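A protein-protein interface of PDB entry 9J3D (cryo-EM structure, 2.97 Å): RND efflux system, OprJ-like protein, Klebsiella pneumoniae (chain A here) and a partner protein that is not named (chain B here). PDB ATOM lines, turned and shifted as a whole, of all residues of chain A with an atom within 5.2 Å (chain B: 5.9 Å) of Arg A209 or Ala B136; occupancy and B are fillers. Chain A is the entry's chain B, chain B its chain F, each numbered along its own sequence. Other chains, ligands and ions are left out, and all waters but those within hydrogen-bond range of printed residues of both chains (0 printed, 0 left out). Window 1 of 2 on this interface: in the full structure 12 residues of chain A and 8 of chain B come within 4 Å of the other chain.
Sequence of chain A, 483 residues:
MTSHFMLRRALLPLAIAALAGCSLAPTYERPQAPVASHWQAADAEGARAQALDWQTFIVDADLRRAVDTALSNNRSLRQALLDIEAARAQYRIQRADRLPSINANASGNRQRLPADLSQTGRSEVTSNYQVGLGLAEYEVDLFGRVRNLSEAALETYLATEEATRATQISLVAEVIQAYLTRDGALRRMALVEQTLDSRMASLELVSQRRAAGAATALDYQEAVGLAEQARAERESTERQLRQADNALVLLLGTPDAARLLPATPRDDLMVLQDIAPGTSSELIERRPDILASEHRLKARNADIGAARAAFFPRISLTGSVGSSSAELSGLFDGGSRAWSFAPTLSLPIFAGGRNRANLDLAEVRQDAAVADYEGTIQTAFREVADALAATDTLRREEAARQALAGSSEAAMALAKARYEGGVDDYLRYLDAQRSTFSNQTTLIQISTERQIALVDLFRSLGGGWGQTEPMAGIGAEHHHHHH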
ATOM      1  N   GLU A 204       2.123  21.702 -33.624  1.00  0.00           N
ATOM      2  CA  GLU A 204       1.991  20.267 -33.401  1.00  0.00           C
ATOM      3  C   GLU A 204       2.748  19.843 -32.153  1.00  0.00           C
ATOM      4  O   GLU A 204       2.238  19.066 -31.334  1.00  0.00           O
ATOM      5  CB  GLU A 204       2.500  19.503 -34.623  1.00  0.00           C
ATOM      6  CG  GLU A 204       2.430  17.992 -34.488  1.00  0.00           C
ATOM      7  CD  GLU A 204       2.962  17.274 -35.713  1.00  0.00           C
ATOM      8  OE1 GLU A 204       3.396  17.958 -36.663  1.00  0.00           O
ATOM      9  OE2 GLU A 204       2.950  16.026 -35.725  1.00  0.00           O
ATOM     10  N   LEU A 205       3.969  20.351 -31.987  1.00  0.00           N
ATOM     11  CA  LEU A 205       4.759  19.988 -30.817  1.00  0.00           C
ATOM     12  C   LEU A 205       4.085  20.457 -29.532  1.00  0.00           C
ATOM     13  O   LEU A 205       4.037  19.724 -28.539  1.00  0.00           O
ATOM     14  CB  LEU A 205       6.163  20.572 -30.939  1.00  0.00           C
ATOM     15  CG  LEU A 205       7.193  19.975 -29.986  1.00  0.00           C
ATOM     16  CD1 LEU A 205       7.488  18.537 -30.369  1.00  0.00           C
ATOM     17  CD2 LEU A 205       8.456  20.805 -30.010  1.00  0.00           C
ATOM     18  N   VAL A 206       3.546  21.677 -29.538  1.00  0.00           N
ATOM     19  CA  VAL A 206       2.904  22.208 -28.338  1.00  0.00           C
ATOM     20  C   VAL A 206       1.623  21.443 -28.030  1.00  0.00           C
ATOM     21  O   VAL A 206       1.302  21.193 -26.863  1.00  0.00           O
ATOM     22  CB  VAL A 206       2.646  23.716 -28.495  1.00  0.00           C
ATOM     23  CG1 VAL A 206       1.781  24.232 -27.362  1.00  0.00           C
ATOM     24  CG2 VAL A 206       3.962  24.470 -28.530  1.00  0.00           C
ATOM     25  N   SER A 207       0.871  21.060 -29.062  1.00  0.00           N
ATOM     26  CA  SER A 207      -0.326  20.255 -28.840  1.00  0.00           C
ATOM     27  C   SER A 207       0.033  18.906 -28.232  1.00  0.00           C
ATOM     28  O   SER A 207      -0.643  18.422 -27.316  1.00  0.00           O
ATOM     29  CB  SER A 207      -1.083  20.073 -30.154  1.00  0.00           C
ATOM     30  OG  SER A 207      -2.283  19.346 -29.955  1.00  0.00           O
ATOM     31  N   GLN A 208       1.104  18.285 -28.731  1.00  0.00           N
ATOM     32  CA  GLN A 208       1.537  17.010 -28.174  1.00  0.00           C
ATOM     33  C   GLN A 208       2.003  17.165 -26.732  1.00  0.00           C
ATOM     34  O   GLN A 208       1.775  16.280 -25.900  1.00  0.00           O
ATOM     35  CB  GLN A 208       2.636  16.407 -29.047  1.00  0.00           C
ATOM     36  CG  GLN A 208       2.110  15.800 -30.340  1.00  0.00           C
ATOM     37  CD  GLN A 208       3.197  15.555 -31.367  1.00  0.00           C
ATOM     38  OE1 GLN A 208       4.385  15.668 -31.070  1.00  0.00           O
ATOM     39  NE2 GLN A 208       2.794  15.218 -32.586  1.00  0.00           N
ATOM     40  N   ARG A 209       2.666  18.281 -26.416  1.00  0.00           N
ATOM     41  CA  ARG A 209       3.058  18.537 -25.032  1.00  0.00           C
ATOM     42  C   ARG A 209       1.841  18.720 -24.134  1.00  0.00           C
ATOM     43  O   ARG A 209       1.808  18.206 -23.011  1.00  0.00           O
ATOM     44  CB  ARG A 209       3.961  19.768 -24.953  1.00  0.00           C
ATOM     45  CG  ARG A 209       5.284  19.608 -25.670  1.00  0.00           C
ATOM     46  CD  ARG A 209       6.387  20.392 -24.989  1.00  0.00           C
ATOM     47  NE  ARG A 209       5.869  21.535 -24.248  1.00  0.00           N
ATOM     48  CZ  ARG A 209       6.524  22.151 -23.276  1.00  0.00           C
ATOM     49  NH1 ARG A 209       7.729  21.757 -22.896  1.00  0.00           N
ATOM     50  NH2 ARG A 209       5.959  23.190 -22.669  1.00  0.00           N
ATOM     51  N   ARG A 210       0.864  19.551 -24.472  1.00  0.00           N
ATOM     52  CA  ARG A 210      -0.359  19.642 -23.632  1.00  0.00           C
ATOM     53  C   ARG A 210      -1.038  18.276 -23.522  1.00  0.00           C
ATOM     54  O   ARG A 210      -1.497  17.979 -22.428  1.00  0.00           O
ATOM     55  CB  ARG A 210      -1.340  20.661 -24.201  1.00  0.00           C
ATOM     56  CG  ARG A 210      -2.659  20.772 -23.457  1.00  0.00           C
ATOM     57  CD  ARG A 210      -3.733  21.187 -24.437  1.00  0.00           C
ATOM     58  NE  ARG A 210      -5.061  21.113 -23.858  1.00  0.00           N
ATOM     59  CZ  ARG A 210      -6.049  21.948 -24.151  1.00  0.00           C
ATOM     60  NH1 ARG A 210      -5.859  22.927 -25.018  1.00  0.00           N
ATOM     61  NH2 ARG A 210      -7.226  21.802 -23.573  1.00  0.00           N
ATOM     62  N   ALA A 211      -1.134  17.477 -24.594  1.00  0.00           N
ATOM     63  CA  ALA A 211      -1.777  16.177 -24.429  1.00  0.00           C
ATOM     64  C   ALA A 211      -1.137  15.374 -23.305  1.00  0.00           C
ATOM     65  O   ALA A 211      -1.822  14.603 -22.627  1.00  0.00           O
ATOM     66  CB  ALA A 211      -1.725  15.395 -25.739  1.00  0.00           C
ATOM     67  N   ALA A 212       0.166  15.543 -23.090  1.00  0.00           N
ATOM     68  CA  ALA A 212       0.865  14.851 -22.016  1.00  0.00           C
ATOM     69  C   ALA A 212       0.802  15.595 -20.690  1.00  0.00           C
ATOM     70  O   ALA A 212       1.312  15.083 -19.690  1.00  0.00           O
ATOM     71  CB  ALA A 212       2.325  14.617 -22.403  1.00  0.00           C
ATOM     72  N   GLY A 213       0.200  16.781 -20.655  1.00  0.00           N
ATOM     73  CA  GLY A 213       0.062  17.527 -19.421  1.00  0.00           C
ATOM     74  C   GLY A 213       1.258  18.358 -19.020  1.00  0.00           C
ATOM     75  O   GLY A 213       1.239  18.956 -17.940  1.00  0.00           O
ATOM     76  N   ALA A 214       2.294  18.421 -19.850  1.00  0.00           N
ATOM     77  CA  ALA A 214       3.483  19.203 -19.543  1.00  0.00           C
ATOM     78  C   ALA A 214       3.348  20.667 -19.935  1.00  0.00           C
ATOM     79  O   ALA A 214       4.243  21.458 -19.627  1.00  0.00           O
ATOM     80  CB  ALA A 214       4.705  18.596 -20.235  1.00  0.00           C
ATOM     81  N   ALA A 215       2.264  21.045 -20.607  1.00  0.00           N
ATOM     82  CA  ALA A 215       2.045  22.418 -21.031  1.00  0.00           C
ATOM     83  C   ALA A 215       0.627  22.842 -20.685  1.00  0.00           C
ATOM     84  O   ALA A 215      -0.300  22.029 -20.683  1.00  0.00           O
ATOM     85  CB  ALA A 215       2.287  22.587 -22.537  1.00  0.00           C
ATOM     86  N   ASP A 219      -0.400  28.056 -23.314  1.00  0.00           N
ATOM     87  CA  ASP A 219       0.664  27.857 -24.291  1.00  0.00           C
ATOM     88  C   ASP A 219       0.112  27.334 -25.611  1.00  0.00           C
ATOM     89  O   ASP A 219       0.543  27.758 -26.691  1.00  0.00           O
ATOM     90  CB  ASP A 219       1.715  26.904 -23.727  1.00  0.00           C
ATOM     91  CG  ASP A 219       2.241  27.355 -22.378  1.00  0.00           C
ATOM     92  OD1 ASP A 219       2.516  28.563 -22.220  1.00  0.00           O
ATOM     93  OD2 ASP A 219       2.376  26.504 -21.474  1.00  0.00           O
ATOM     94  N   ASP A 425      15.641  22.596 -26.401  1.00  0.00           N
ATOM     95  CA  ASP A 425      14.468  21.906 -26.911  1.00  0.00           C
ATOM     96  C   ASP A 425      14.236  22.242 -28.383  1.00  0.00           C
ATOM     97  O   ASP A 425      14.923  23.072 -28.981  1.00  0.00           O
ATOM     98  CB  ASP A 425      13.235  22.262 -26.080  1.00  0.00           C
ATOM     99  CG  ASP A 425      13.051  23.761 -25.912  1.00  0.00           C
ATOM    100  OD1 ASP A 425      13.699  24.538 -26.644  1.00  0.00           O
ATOM    101  OD2 ASP A 425      12.252  24.166 -25.040  1.00  0.00           O
ATOM    102  N   LEU A 427      11.655  23.757 -29.510  1.00  0.00           N
ATOM    103  CA  LEU A 427      11.024  25.065 -29.633  1.00  0.00           C
ATOM    104  C   LEU A 427      12.051  26.150 -29.936  1.00  0.00           C
ATOM    105  O   LEU A 427      11.798  27.037 -30.757  1.00  0.00           O
ATOM    106  CB  LEU A 427      10.253  25.410 -28.359  1.00  0.00           C
ATOM    107  CG  LEU A 427       8.968  24.643 -28.020  1.00  0.00           C
ATOM    108  CD1 LEU A 427       8.026  24.603 -29.213  1.00  0.00           C
ATOM    109  CD2 LEU A 427       9.247  23.246 -27.485  1.00  0.00           C
ATOM    110  N   LEU B 131       7.597  12.320 -24.559  1.00  0.00           N
ATOM    111  CA  LEU B 131       7.854  13.644 -25.114  1.00  0.00           C
ATOM    112  C   LEU B 131       9.287  13.771 -25.614  1.00  0.00           C
ATOM    113  O   LEU B 131       9.547  14.483 -26.591  1.00  0.00           O
ATOM    114  CB  LEU B 131       7.554  14.717 -24.071  1.00  0.00           C
ATOM    115  CG  LEU B 131       6.086  14.883 -23.681  1.00  0.00           C
ATOM    116  CD1 LEU B 131       5.933  15.925 -22.588  1.00  0.00           C
ATOM    117  CD2 LEU B 131       5.250  15.249 -24.892  1.00  0.00           C
ATOM    118  N   VAL B 132      10.235  13.102 -24.956  1.00  0.00           N
ATOM    119  CA  VAL B 132      11.627  13.202 -25.384  1.00  0.00           C
ATOM    120  C   VAL B 132      11.840  12.487 -26.713  1.00  0.00           C
ATOM    121  O   VAL B 132      12.718  12.868 -27.495  1.00  0.00           O
ATOM    122  CB  VAL B 132      12.566  12.670 -24.285  1.00  0.00           C
ATOM    123  CG1 VAL B 132      12.505  11.155 -24.201  1.00  0.00           C
ATOM    124  CG2 VAL B 132      13.988  13.138 -24.532  1.00  0.00           C
ATOM    125  N   LYS B 133      11.049  11.450 -26.997  1.00  0.00           N
ATOM    126  CA  LYS B 133      11.167  10.754 -28.272  1.00  0.00           C
ATOM    127  C   LYS B 133      10.709  11.613 -29.441  1.00  0.00           C
ATOM    128  O   LYS B 133      11.203  11.434 -30.558  1.00  0.00           O
ATOM    129  CB  LYS B 133      10.368   9.451 -28.236  1.00  0.00           C
ATOM    130  CG  LYS B 133      11.134   8.273 -27.659  1.00  0.00           C
ATOM    131  CD  LYS B 133      10.287   7.491 -26.669  1.00  0.00           C
ATOM    132  CE  LYS B 133      11.153   6.793 -25.637  1.00  0.00           C
ATOM    133  NZ  LYS B 133      11.337   7.626 -24.419  1.00  0.00           N
ATOM    134  N   ILE B 134       9.777  12.533 -29.212  1.00  0.00           N
ATOM    135  CA  ILE B 134       9.317  13.460 -30.234  1.00  0.00           C
ATOM    136  C   ILE B 134      10.002  14.818 -30.092  1.00  0.00           C
ATOM    137  O   ILE B 134       9.551  15.804 -30.669  1.00  0.00           O
ATOM    138  CB  ILE B 134       7.786  13.602 -30.207  1.00  0.00           C
ATOM    139  CG1 ILE B 134       7.314  13.939 -28.793  1.00  0.00           C
ATOM    140  CG2 ILE B 134       7.130  12.327 -30.703  1.00  0.00           C
ATOM    141  CD1 ILE B 134       5.830  14.182 -28.680  1.00  0.00           C
ATOM    142  N   ASP B 135      11.083  14.874 -29.314  1.00  0.00           N
ATOM    143  CA  ASP B 135      11.882  16.079 -29.104  1.00  0.00           C
ATOM    144  C   ASP B 135      11.072  17.223 -28.507  1.00  0.00           C
ATOM    145  O   ASP B 135      11.409  18.393 -28.704  1.00  0.00           O
ATOM    146  CB  ASP B 135      12.555  16.529 -30.403  1.00  0.00           C
ATOM    147  CG  ASP B 135      13.434  15.452 -31.003  1.00  0.00           C
ATOM    148  OD1 ASP B 135      14.364  14.987 -30.311  1.00  0.00           O
ATOM    149  OD2 ASP B 135      13.195  15.067 -32.167  1.00  0.00           O
ATOM    150  N   ALA B 136      10.006  16.909 -27.774  1.00  0.00           N
ATOM    151  CA  ALA B 136       9.203  17.935 -27.125  1.00  0.00           C
ATOM    152  C   ALA B 136       9.914  18.587 -25.949  1.00  0.00           C
ATOM    153  O   ALA B 136       9.611  19.739 -25.627  1.00  0.00           O
ATOM    154  CB  ALA B 136       7.875  17.342 -26.659  1.00  0.00           C
ATOM    155  N   VAL B 137      10.840  17.881 -25.300  1.00  0.00           N
ATOM    156  CA  VAL B 137      11.646  18.436 -24.221  1.00  0.00           C
ATOM    157  C   VAL B 137      13.106  18.121 -24.507  1.00  0.00           C
ATOM    158  O   VAL B 137      13.435  17.168 -25.216  1.00  0.00           O
ATOM    159  CB  VAL B 137      11.244  17.888 -22.835  1.00  0.00           C
ATOM    160  CG1 VAL B 137       9.834  18.322 -22.482  1.00  0.00           C
ATOM    161  CG2 VAL B 137      11.364  16.376 -22.808  1.00  0.00           C
ATOM    162  N   SER B 138      13.987  18.944 -23.948  1.00  0.00           N
ATOM    163  CA  SER B 138      15.413  18.756 -24.162  1.00  0.00           C
ATOM    164  C   SER B 138      15.896  17.484 -23.477  1.00  0.00           C
ATOM    165  O   SER B 138      15.331  17.037 -22.476  1.00  0.00           O
ATOM    166  CB  SER B 138      16.194  19.960 -23.641  1.00  0.00           C
ATOM    167  OG  SER B 138      16.347  19.897 -22.235  1.00  0.00           O
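OE2 of Glu A204 lies within hydrogen-bond range of NE2 of Gln A208 (3.2 Å). The backbone NH of Ala A214 is in hydrogen-bond range of the backbone carbonyl oxygen of Arg A209. The backbone NH (N) of Ala B136 sits at hydrogen-bond distance from the backbone carbonyl oxygen (O) of Leu B131 (2.7 Å).
Hydrophobic or aromatic side chains of chain A within 4 Å of the printed part of chain B: Leu A205, Ala A212, Ala A214 and Leu A427. Printed residues of chain B that touch a printed residue of chain A: Leu B131, Ile B134, Ala B136 and Ser B138. Hydrophobic or aromatic side chains of chain B within 4 Å of the printed part of chain A: Leu B131, Ile B134 and Ala B136. Among the printed residues, no Asp or Glu carboxylate lies within 4 Å of a Lys or Arg side-chain nitrogen of the other chain.
Among the printed residues, pairs that only touch across the chains: Leu A205 with Ile B134, Leu A205 with Ala B136, Gln A208 with Leu B131, Gln A208 with Ile B134, Arg A209 with Leu B131, Arg A209 with Ala B136, Ala A212 with Leu B131, Ala A214 with Leu B131, Asp A425 with Ser B138 and Leu A427 with Ala B136.
Printed residues of chain B within 4 Å of Gln A208: Leu B131 (3.8 Å) and Ile B134 (3.2 Å). Arg A209 touches two residues of chain B. Ala A215 touches none of the printed residues of chain B. Printed residues of chain B within 4 Å of Asp A425: Ser B138. Of the printed residues of chain A, Ile B134 touches Leu A205 and Gln A208. Printed residues of chain A within 4 Å of Ala B136: Leu A205 (3.7 Å), Arg A209 (3.4 Å) and Leu A427 (3.99 Å). Val B137 touches none of the printed residues of chain A. Printed residues of chain A within 4 Å of Ser B138: Asp A425 (3.9 Å). The nearest residue of chain B that does not touch Arg A209 is Val B137 (4.05 Å). The nearest printed residue of chain A that does not touch Ala B136 is Asp A425 (4.4 Å).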
